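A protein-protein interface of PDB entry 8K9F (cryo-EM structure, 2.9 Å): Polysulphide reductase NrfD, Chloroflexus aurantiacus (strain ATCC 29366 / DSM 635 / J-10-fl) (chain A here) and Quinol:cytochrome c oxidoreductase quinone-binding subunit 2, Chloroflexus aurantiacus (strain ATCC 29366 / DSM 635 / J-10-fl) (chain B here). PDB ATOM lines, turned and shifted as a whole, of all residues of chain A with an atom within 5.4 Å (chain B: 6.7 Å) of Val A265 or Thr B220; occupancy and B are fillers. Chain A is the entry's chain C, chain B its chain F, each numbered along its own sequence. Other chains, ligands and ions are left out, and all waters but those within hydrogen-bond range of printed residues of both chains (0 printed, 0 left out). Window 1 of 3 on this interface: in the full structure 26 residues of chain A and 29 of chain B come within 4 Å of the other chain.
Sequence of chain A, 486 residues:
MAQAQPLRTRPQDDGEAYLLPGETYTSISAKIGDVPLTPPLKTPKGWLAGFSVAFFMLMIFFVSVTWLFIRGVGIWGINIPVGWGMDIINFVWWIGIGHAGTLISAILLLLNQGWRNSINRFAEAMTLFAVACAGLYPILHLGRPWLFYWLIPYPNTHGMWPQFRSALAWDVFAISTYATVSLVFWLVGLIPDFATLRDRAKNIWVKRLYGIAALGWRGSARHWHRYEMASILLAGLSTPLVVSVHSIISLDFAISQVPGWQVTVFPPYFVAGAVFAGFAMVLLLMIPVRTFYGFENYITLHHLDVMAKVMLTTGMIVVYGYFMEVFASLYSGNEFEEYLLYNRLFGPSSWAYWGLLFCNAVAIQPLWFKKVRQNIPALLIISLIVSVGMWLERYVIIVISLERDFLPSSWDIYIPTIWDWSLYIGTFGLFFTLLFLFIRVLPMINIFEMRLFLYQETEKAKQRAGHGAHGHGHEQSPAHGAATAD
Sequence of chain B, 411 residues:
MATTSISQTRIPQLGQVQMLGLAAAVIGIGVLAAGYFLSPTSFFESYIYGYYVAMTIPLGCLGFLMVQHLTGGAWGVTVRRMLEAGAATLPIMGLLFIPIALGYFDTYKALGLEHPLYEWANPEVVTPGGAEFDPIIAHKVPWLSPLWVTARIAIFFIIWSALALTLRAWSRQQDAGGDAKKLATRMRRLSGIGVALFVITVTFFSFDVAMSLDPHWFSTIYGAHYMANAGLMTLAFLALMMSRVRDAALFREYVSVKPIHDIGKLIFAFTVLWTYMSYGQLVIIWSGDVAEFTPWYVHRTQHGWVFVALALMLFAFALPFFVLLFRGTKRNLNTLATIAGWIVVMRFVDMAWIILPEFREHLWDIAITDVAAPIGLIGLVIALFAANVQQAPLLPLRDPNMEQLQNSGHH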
ATOM      1  N   VAL A 263      32.568 -18.421  -1.685  1.00  0.00           N
ATOM      2  CA  VAL A 263      31.762 -17.435  -0.977  1.00  0.00           C
ATOM      3  C   VAL A 263      30.377 -18.038  -0.799  1.00  0.00           C
ATOM      4  O   VAL A 263      29.778 -18.507  -1.771  1.00  0.00           O
ATOM      5  CB  VAL A 263      31.678 -16.091  -1.729  1.00  0.00           C
ATOM      6  CG1 VAL A 263      30.872 -15.096  -0.939  1.00  0.00           C
ATOM      7  CG2 VAL A 263      33.056 -15.512  -2.023  1.00  0.00           C
ATOM      8  N   THR A 264      29.874 -18.035   0.437  1.00  0.00           N
ATOM      9  CA  THR A 264      28.597 -18.680   0.725  1.00  0.00           C
ATOM     10  C   THR A 264      27.410 -17.933   0.133  1.00  0.00           C
ATOM     11  O   THR A 264      26.362 -18.545  -0.084  1.00  0.00           O
ATOM     12  CB  THR A 264      28.403 -18.829   2.229  1.00  0.00           C
ATOM     13  OG1 THR A 264      28.835 -17.632   2.887  1.00  0.00           O
ATOM     14  CG2 THR A 264      29.206 -20.003   2.747  1.00  0.00           C
ATOM     15  N   VAL A 265      27.552 -16.633  -0.154  1.00  0.00           N
ATOM     16  CA  VAL A 265      26.443 -15.859  -0.708  1.00  0.00           C
ATOM     17  C   VAL A 265      26.218 -16.142  -2.182  1.00  0.00           C
ATOM     18  O   VAL A 265      25.197 -15.709  -2.725  1.00  0.00           O
ATOM     19  CB  VAL A 265      26.670 -14.347  -0.485  1.00  0.00           C
ATOM     20  CG1 VAL A 265      27.913 -13.834  -1.209  1.00  0.00           C
ATOM     21  CG2 VAL A 265      25.421 -13.538  -0.832  1.00  0.00           C
ATOM     22  N   PHE A 266      27.112 -16.899  -2.818  1.00  0.00           N
ATOM     23  CA  PHE A 266      27.131 -17.011  -4.276  1.00  0.00           C
ATOM     24  C   PHE A 266      25.867 -17.556  -4.950  1.00  0.00           C
ATOM     25  O   PHE A 266      25.529 -17.021  -6.018  1.00  0.00           O
ATOM     26  CB  PHE A 266      28.358 -17.823  -4.708  1.00  0.00           C
ATOM     27  CG  PHE A 266      29.526 -16.976  -5.115  1.00  0.00           C
ATOM     28  CD1 PHE A 266      29.638 -15.668  -4.667  1.00  0.00           C
ATOM     29  CD2 PHE A 266      30.505 -17.481  -5.944  1.00  0.00           C
ATOM     30  CE1 PHE A 266      30.714 -14.884  -5.035  1.00  0.00           C
ATOM     31  CE2 PHE A 266      31.579 -16.702  -6.318  1.00  0.00           C
ATOM     32  CZ  PHE A 266      31.684 -15.402  -5.864  1.00  0.00           C
ATOM     33  N   PRO A 267      25.145 -18.574  -4.455  1.00  0.00           N
ATOM     34  CA  PRO A 267      23.959 -19.034  -5.212  1.00  0.00           C
ATOM     35  C   PRO A 267      22.815 -18.023  -5.242  1.00  0.00           C
ATOM     36  O   PRO A 267      22.303 -17.770  -6.345  1.00  0.00           O
ATOM     37  CB  PRO A 267      23.578 -20.361  -4.526  1.00  0.00           C
ATOM     38  CG  PRO A 267      24.821 -20.822  -3.919  1.00  0.00           C
ATOM     39  CD  PRO A 267      25.500 -19.589  -3.440  1.00  0.00           C
ATOM     40  N   PRO A 268      22.383 -17.385  -4.128  1.00  0.00           N
ATOM     41  CA  PRO A 268      21.385 -16.313  -4.311  1.00  0.00           C
ATOM     42  C   PRO A 268      21.936 -15.085  -5.002  1.00  0.00           C
ATOM     43  O   PRO A 268      21.187 -14.395  -5.704  1.00  0.00           O
ATOM     44  CB  PRO A 268      20.935 -15.991  -2.880  1.00  0.00           C
ATOM     45  CG  PRO A 268      21.264 -17.178  -2.118  1.00  0.00           C
ATOM     46  CD  PRO A 268      22.570 -17.585  -2.673  1.00  0.00           C
ATOM     47  N   TYR A 269      23.231 -14.814  -4.866  1.00  0.00           N
ATOM     48  CA  TYR A 269      23.806 -13.643  -5.514  1.00  0.00           C
ATOM     49  C   TYR A 269      23.954 -13.859  -7.017  1.00  0.00           C
ATOM     50  O   TYR A 269      23.697 -12.941  -7.802  1.00  0.00           O
ATOM     51  CB  TYR A 269      25.128 -13.309  -4.833  1.00  0.00           C
ATOM     52  CG  TYR A 269      26.159 -12.566  -5.619  1.00  0.00           C
ATOM     53  CD1 TYR A 269      25.953 -11.255  -6.020  1.00  0.00           C
ATOM     54  CD2 TYR A 269      27.370 -13.168  -5.916  1.00  0.00           C
ATOM     55  CE1 TYR A 269      26.925 -10.575  -6.725  1.00  0.00           C
ATOM     56  CE2 TYR A 269      28.332 -12.507  -6.616  1.00  0.00           C
ATOM     57  CZ  TYR A 269      28.112 -11.213  -7.013  1.00  0.00           C
ATOM     58  OH  TYR A 269      29.097 -10.572  -7.702  1.00  0.00           O
ATOM     59  N   PHE A 270      24.313 -15.073  -7.445  1.00  0.00           N
ATOM     60  CA  PHE A 270      24.315 -15.367  -8.877  1.00  0.00           C
ATOM     61  C   PHE A 270      22.907 -15.458  -9.436  1.00  0.00           C
ATOM     62  O   PHE A 270      22.690 -15.117 -10.604  1.00  0.00           O
ATOM     63  CB  PHE A 270      25.034 -16.673  -9.179  1.00  0.00           C
ATOM     64  CG  PHE A 270      26.515 -16.536  -9.388  1.00  0.00           C
ATOM     65  CD1 PHE A 270      27.318 -15.940  -8.431  1.00  0.00           C
ATOM     66  CD2 PHE A 270      27.108 -17.046 -10.528  1.00  0.00           C
ATOM     67  CE1 PHE A 270      28.679 -15.839  -8.618  1.00  0.00           C
ATOM     68  CE2 PHE A 270      28.467 -16.945 -10.721  1.00  0.00           C
ATOM     69  CZ  PHE A 270      29.253 -16.341  -9.768  1.00  0.00           C
ATOM     70  N   TYR A 320      24.063  -5.622  -2.701  1.00  0.00           N
ATOM     71  CA  TYR A 320      24.187  -6.262  -1.396  1.00  0.00           C
ATOM     72  C   TYR A 320      25.185  -7.412  -1.439  1.00  0.00           C
ATOM     73  O   TYR A 320      25.918  -7.638  -0.474  1.00  0.00           O
ATOM     74  CB  TYR A 320      22.806  -6.748  -0.943  1.00  0.00           C
ATOM     75  CG  TYR A 320      22.786  -7.864   0.082  1.00  0.00           C
ATOM     76  CD1 TYR A 320      22.914  -7.586   1.435  1.00  0.00           C
ATOM     77  CD2 TYR A 320      22.603  -9.188  -0.301  1.00  0.00           C
ATOM     78  CE1 TYR A 320      22.875  -8.590   2.377  1.00  0.00           C
ATOM     79  CE2 TYR A 320      22.576 -10.201   0.631  1.00  0.00           C
ATOM     80  CZ  TYR A 320      22.710  -9.897   1.966  1.00  0.00           C
ATOM     81  OH  TYR A 320      22.677 -10.912   2.887  1.00  0.00           O
ATOM     82  N   GLY A 321      25.215  -8.158  -2.546  1.00  0.00           N
ATOM     83  CA  GLY A 321      26.203  -9.221  -2.691  1.00  0.00           C
ATOM     84  C   GLY A 321      27.626  -8.698  -2.782  1.00  0.00           C
ATOM     85  O   GLY A 321      28.557  -9.307  -2.239  1.00  0.00           O
ATOM     86  N   MET A 324      28.519  -7.881   0.655  1.00  0.00           N
ATOM     87  CA  MET A 324      28.871  -9.111   1.362  1.00  0.00           C
ATOM     88  C   MET A 324      30.284  -9.565   1.035  1.00  0.00           C
ATOM     89  O   MET A 324      30.982 -10.091   1.905  1.00  0.00           O
ATOM     90  CB  MET A 324      27.874 -10.221   1.026  1.00  0.00           C
ATOM     91  CG  MET A 324      26.453  -9.942   1.488  1.00  0.00           C
ATOM     92  SD  MET A 324      26.317  -9.806   3.279  1.00  0.00           S
ATOM     93  CE  MET A 324      26.199  -8.030   3.476  1.00  0.00           C
ATOM     94  N   GLU A 325      30.716  -9.396  -0.217  1.00  0.00           N
ATOM     95  CA  GLU A 325      32.101  -9.710  -0.564  1.00  0.00           C
ATOM     96  C   GLU A 325      33.080  -8.785   0.149  1.00  0.00           C
ATOM     97  O   GLU A 325      34.113  -9.241   0.659  1.00  0.00           O
ATOM     98  CB  GLU A 325      32.303  -9.618  -2.072  1.00  0.00           C
ATOM     99  CG  GLU A 325      31.757 -10.787  -2.846  1.00  0.00           C
ATOM    100  CD  GLU A 325      31.382 -10.404  -4.256  1.00  0.00           C
ATOM    101  OE1 GLU A 325      32.002  -9.474  -4.817  1.00  0.00           O
ATOM    102  OE2 GLU A 325      30.463 -11.034  -4.805  1.00  0.00           O
ATOM    103  N   ALA A 328      33.151  -9.840   3.734  1.00  0.00           N
ATOM    104  CA  ALA A 328      33.908 -11.077   3.895  1.00  0.00           C
ATOM    105  C   ALA A 328      35.402 -10.820   3.835  1.00  0.00           C
ATOM    106  O   ALA A 328      36.178 -11.465   4.541  1.00  0.00           O
ATOM    107  CB  ALA A 328      33.519 -12.079   2.816  1.00  0.00           C
ATOM    108  N   THR B 203      20.579  -8.264   7.831  1.00  0.00           N
ATOM    109  CA  THR B 203      21.761  -9.083   7.597  1.00  0.00           C
ATOM    110  C   THR B 203      22.881  -8.707   8.559  1.00  0.00           C
ATOM    111  O   THR B 203      23.511  -9.582   9.170  1.00  0.00           O
ATOM    112  CB  THR B 203      22.212  -8.924   6.150  1.00  0.00           C
ATOM    113  OG1 THR B 203      21.179  -9.395   5.280  1.00  0.00           O
ATOM    114  CG2 THR B 203      23.463  -9.718   5.900  1.00  0.00           C
ATOM    115  N   PHE B 207      24.469 -10.828  11.707  1.00  0.00           N
ATOM    116  CA  PHE B 207      25.915 -10.888  11.916  1.00  0.00           C
ATOM    117  C   PHE B 207      26.279 -10.585  13.368  1.00  0.00           C
ATOM    118  O   PHE B 207      26.754 -11.476  14.079  1.00  0.00           O
ATOM    119  CB  PHE B 207      26.635  -9.923  10.976  1.00  0.00           C
ATOM    120  CG  PHE B 207      26.702 -10.395   9.558  1.00  0.00           C
ATOM    121  CD1 PHE B 207      26.631 -11.741   9.260  1.00  0.00           C
ATOM    122  CD2 PHE B 207      26.767  -9.488   8.518  1.00  0.00           C
ATOM    123  CE1 PHE B 207      26.673 -12.179   7.956  1.00  0.00           C
ATOM    124  CE2 PHE B 207      26.823  -9.922   7.209  1.00  0.00           C
ATOM    125  CZ  PHE B 207      26.768 -11.269   6.928  1.00  0.00           C
ATOM    126  N   MET B 211      26.407 -14.376  14.397  1.00  0.00           N
ATOM    127  CA  MET B 211      27.615 -14.839  13.736  1.00  0.00           C
ATOM    128  C   MET B 211      28.872 -14.334  14.420  1.00  0.00           C
ATOM    129  O   MET B 211      29.954 -14.879  14.185  1.00  0.00           O
ATOM    130  CB  MET B 211      27.597 -14.394  12.278  1.00  0.00           C
ATOM    131  CG  MET B 211      28.271 -15.336  11.319  1.00  0.00           C
ATOM    132  SD  MET B 211      28.805 -14.441   9.863  1.00  0.00           S
ATOM    133  CE  MET B 211      29.691 -13.087  10.625  1.00  0.00           C
ATOM    134  N   PHE B 218      32.789 -17.038   9.674  1.00  0.00           N
ATOM    135  CA  PHE B 218      31.880 -16.111   9.022  1.00  0.00           C
ATOM    136  C   PHE B 218      31.039 -16.893   8.027  1.00  0.00           C
ATOM    137  O   PHE B 218      31.389 -18.003   7.623  1.00  0.00           O
ATOM    138  CB  PHE B 218      32.661 -14.906   8.410  1.00  0.00           C
ATOM    139  CG  PHE B 218      33.487 -15.201   7.151  1.00  0.00           C
ATOM    140  CD1 PHE B 218      32.909 -15.459   5.899  1.00  0.00           C
ATOM    141  CD2 PHE B 218      34.842 -14.944   7.175  1.00  0.00           C
ATOM    142  CE1 PHE B 218      33.679 -15.659   4.783  1.00  0.00           C
ATOM    143  CE2 PHE B 218      35.620 -15.159   6.057  1.00  0.00           C
ATOM    144  CZ  PHE B 218      35.035 -15.488   4.857  1.00  0.00           C
ATOM    145  N   SER B 219      29.935 -16.285   7.616  1.00  0.00           N
ATOM    146  CA  SER B 219      29.231 -16.706   6.419  1.00  0.00           C
ATOM    147  C   SER B 219      28.613 -15.478   5.784  1.00  0.00           C
ATOM    148  O   SER B 219      28.096 -14.606   6.482  1.00  0.00           O
ATOM    149  CB  SER B 219      28.146 -17.737   6.717  1.00  0.00           C
ATOM    150  OG  SER B 219      27.855 -18.512   5.570  1.00  0.00           O
ATOM    151  N   THR B 220      28.677 -15.402   4.465  1.00  0.00           N
ATOM    152  CA  THR B 220      28.018 -14.315   3.764  1.00  0.00           C
ATOM    153  C   THR B 220      26.569 -14.627   3.438  1.00  0.00           C
ATOM    154  O   THR B 220      25.790 -13.705   3.179  1.00  0.00           O
ATOM    155  CB  THR B 220      28.783 -13.985   2.490  1.00  0.00           C
ATOM    156  OG1 THR B 220      29.069 -15.198   1.787  1.00  0.00           O
ATOM    157  CG2 THR B 220      30.061 -13.285   2.820  1.00  0.00           C
ATOM    158  N   ILE B 221      26.191 -15.905   3.463  1.00  0.00           N
ATOM    159  CA  ILE B 221      24.789 -16.291   3.351  1.00  0.00           C
ATOM    160  C   ILE B 221      24.077 -16.241   4.690  1.00  0.00           C
ATOM    161  O   ILE B 221      22.849 -16.400   4.740  1.00  0.00           O
ATOM    162  CB  ILE B 221      24.718 -17.682   2.699  1.00  0.00           C
ATOM    163  CG1 ILE B 221      23.421 -17.848   1.905  1.00  0.00           C
ATOM    164  CG2 ILE B 221      24.873 -18.742   3.731  1.00  0.00           C
ATOM    165  CD1 ILE B 221      23.166 -16.725   0.961  1.00  0.00           C
ATOM    166  N   TYR B 222      24.792 -15.958   5.755  1.00  0.00           N
ATOM    167  CA  TYR B 222      24.120 -15.814   7.019  1.00  0.00           C
ATOM    168  C   TYR B 222      23.340 -14.542   6.793  1.00  0.00           C
ATOM    169  O   TYR B 222      23.694 -13.748   5.928  1.00  0.00           O
ATOM    170  CB  TYR B 222      25.172 -15.601   8.091  1.00  0.00           C
ATOM    171  CG  TYR B 222      24.864 -16.214   9.429  1.00  0.00           C
ATOM    172  CD1 TYR B 222      23.996 -15.603  10.310  1.00  0.00           C
ATOM    173  CD2 TYR B 222      25.467 -17.388   9.819  1.00  0.00           C
ATOM    174  CE1 TYR B 222      23.717 -16.160  11.536  1.00  0.00           C
ATOM    175  CE2 TYR B 222      25.202 -17.952  11.041  1.00  0.00           C
ATOM    176  CZ  TYR B 222      24.329 -17.335  11.895  1.00  0.00           C
ATOM    177  OH  TYR B 222      24.072 -17.907  13.109  1.00  0.00           O
ATOM    178  N   GLY B 223      22.331 -14.282   7.580  1.00  0.00           N
ATOM    179  CA  GLY B 223      21.497 -13.117   7.375  1.00  0.00           C
ATOM    180  C   GLY B 223      20.438 -13.366   6.324  1.00  0.00           C
ATOM    181  O   GLY B 223      19.250 -13.181   6.594  1.00  0.00           O
ATOM    182  N   ALA B 224      20.848 -13.777   5.121  1.00  0.00           N
ATOM    183  CA  ALA B 224      19.886 -14.291   4.152  1.00  0.00           C
ATOM    184  C   ALA B 224      19.285 -15.609   4.633  1.00  0.00           C
ATOM    185  O   ALA B 224      18.103 -15.893   4.393  1.00  0.00           O
ATOM    186  CB  ALA B 224      20.554 -14.466   2.791  1.00  0.00           C
ATOM    187  N   HIS B 225      20.097 -16.426   5.303  1.00  0.00           N
ATOM    188  CA  HIS B 225      19.571 -17.569   6.036  1.00  0.00           C
ATOM    189  C   HIS B 225      18.627 -17.104   7.134  1.00  0.00           C
ATOM    190  O   HIS B 225      17.535 -17.664   7.315  1.00  0.00           O
ATOM    191  CB  HIS B 225      20.737 -18.369   6.615  1.00  0.00           C
ATOM    192  CG  HIS B 225      20.327 -19.564   7.412  1.00  0.00           C
ATOM    193  ND1 HIS B 225      20.015 -19.498   8.753  1.00  0.00           N
ATOM    194  CD2 HIS B 225      20.217 -20.868   7.066  1.00  0.00           C
ATOM    195  CE1 HIS B 225      19.706 -20.704   9.190  1.00  0.00           C
ATOM    196  NE2 HIS B 225      19.829 -21.555   8.189  1.00  0.00           N
ATOM    197  N   TYR B 276      16.936 -24.293   0.576  1.00  0.00           N
ATOM    198  CA  TYR B 276      17.884 -23.963  -0.477  1.00  0.00           C
ATOM    199  C   TYR B 276      19.051 -23.157   0.075  1.00  0.00           C
ATOM    200  O   TYR B 276      20.204 -23.403  -0.286  1.00  0.00           O
ATOM    201  CB  TYR B 276      17.153 -23.198  -1.576  1.00  0.00           C
ATOM    202  CG  TYR B 276      17.994 -22.251  -2.387  1.00  0.00           C
ATOM    203  CD1 TYR B 276      18.983 -22.723  -3.241  1.00  0.00           C
ATOM    204  CD2 TYR B 276      17.790 -20.879  -2.308  1.00  0.00           C
ATOM    205  CE1 TYR B 276      19.742 -21.859  -3.982  1.00  0.00           C
ATOM    206  CE2 TYR B 276      18.548 -20.008  -3.049  1.00  0.00           C
ATOM    207  CZ  TYR B 276      19.521 -20.508  -3.887  1.00  0.00           C
ATOM    208  OH  TYR B 276      20.281 -19.652  -4.634  1.00  0.00           O
ATOM    209  N   ILE B 284      28.565 -25.557   0.021  1.00  0.00           N
ATOM    210  CA  ILE B 284      29.714 -24.700  -0.250  1.00  0.00           C
ATOM    211  C   ILE B 284      30.825 -24.977   0.747  1.00  0.00           C
ATOM    212  O   ILE B 284      31.986 -25.176   0.368  1.00  0.00           O
ATOM    213  CB  ILE B 284      29.288 -23.224  -0.229  1.00  0.00           C
ATOM    214  CG1 ILE B 284      28.637 -22.865  -1.550  1.00  0.00           C
ATOM    215  CG2 ILE B 284      30.466 -22.291   0.033  1.00  0.00           C
ATOM    216  CD1 ILE B 284      27.894 -21.588  -1.497  1.00  0.00           C
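Val A265 touches just these residues of chain B: Thr B220 (2.9 Å) and Ile B221 (3.8 Å).
Printed residues of chain B within 4 Å of Pro A267: Tyr B276 and Ile B284.
Of the printed residues of chain B, Tyr A320 touches Thr B203 (3.2 Å).
Printed residues of chain B within 4 Å of Ala A328: Thr B220.
Of chain A, only Val A263, Thr A264, Val A265, Met A324 and Ala A328 come within 4 Å of Thr B220.
Tyr B222 touches none of the printed residues of chain A.
Gly B223 touches none of the printed residues of chain A.
Of the printed residues of chain A, Tyr B276 touches Pro A267 and Pro A268.
Of the printed residues of chain A, Ile B284 touches Val A263, Thr A264 and Pro A267.
The nearest residue of chain B that does not touch Val A265 is Ile B284 (5.1 Å).
The nearest printed residue of chain A that does not touch Thr B203 is Val A265 (8.0 Å).
Among the printed residues, pairs that only touch across the chains: Val A263 with Thr B220, Val A263 with Ile B284, Thr A264 with Ile B284, Val A265 with Ile B221, Pro A267 with Ile B284, Pro A268 with Ile B221, Met A324 with Thr B203, Met A324 with Phe B207, Met A324 with Thr B220 and Ala A328 with Thr B220.
Printed residues of chain A that touch a printed residue of chain B: Val A263, Thr A264, Val A265, Pro A267, Pro A268, Tyr A320, Met A324 and Ala A328.
Hydrophobic or aromatic side chains of chain A within 4 Å of the printed part of chain B: Val A263, Val A265, Pro A267, Pro A268, Tyr A320, Met A324 and Ala A328.
Of the 13 printed residues of chain B, 7 touch a printed residue of chain A.
OG1 of Thr B220 is in hydrogen-bond range of N of Val A265 (2.9 Å).
The backbone NH (N) of Ile B221 is in hydrogen-bond range of the side-chain hydroxyl (OG1) of Thr A264, 3.2 Å away.
The side-chain hydroxyl (OH) of Tyr B276 lies close to the backbone carbonyl oxygen (O) of Pro A267.
OG1 of Thr A264 lies within hydrogen-bond range of OG of Ser B219 (3.0 Å).
The side-chain hydroxyl of Thr B220 sits at hydrogen-bond distance from the side-chain hydroxyl of Thr A264.
OH of Tyr A320 sits at hydrogen-bond distance from OG1 of Thr B203 (3.2 Å).
The backbone nitrogen (N) of Pro A268 sits close to the side-chain hydroxyl (OH) of Tyr B276.
N of Ser B219 is in hydrogen-bond range of SD of Met B211, 3.1 Å away.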
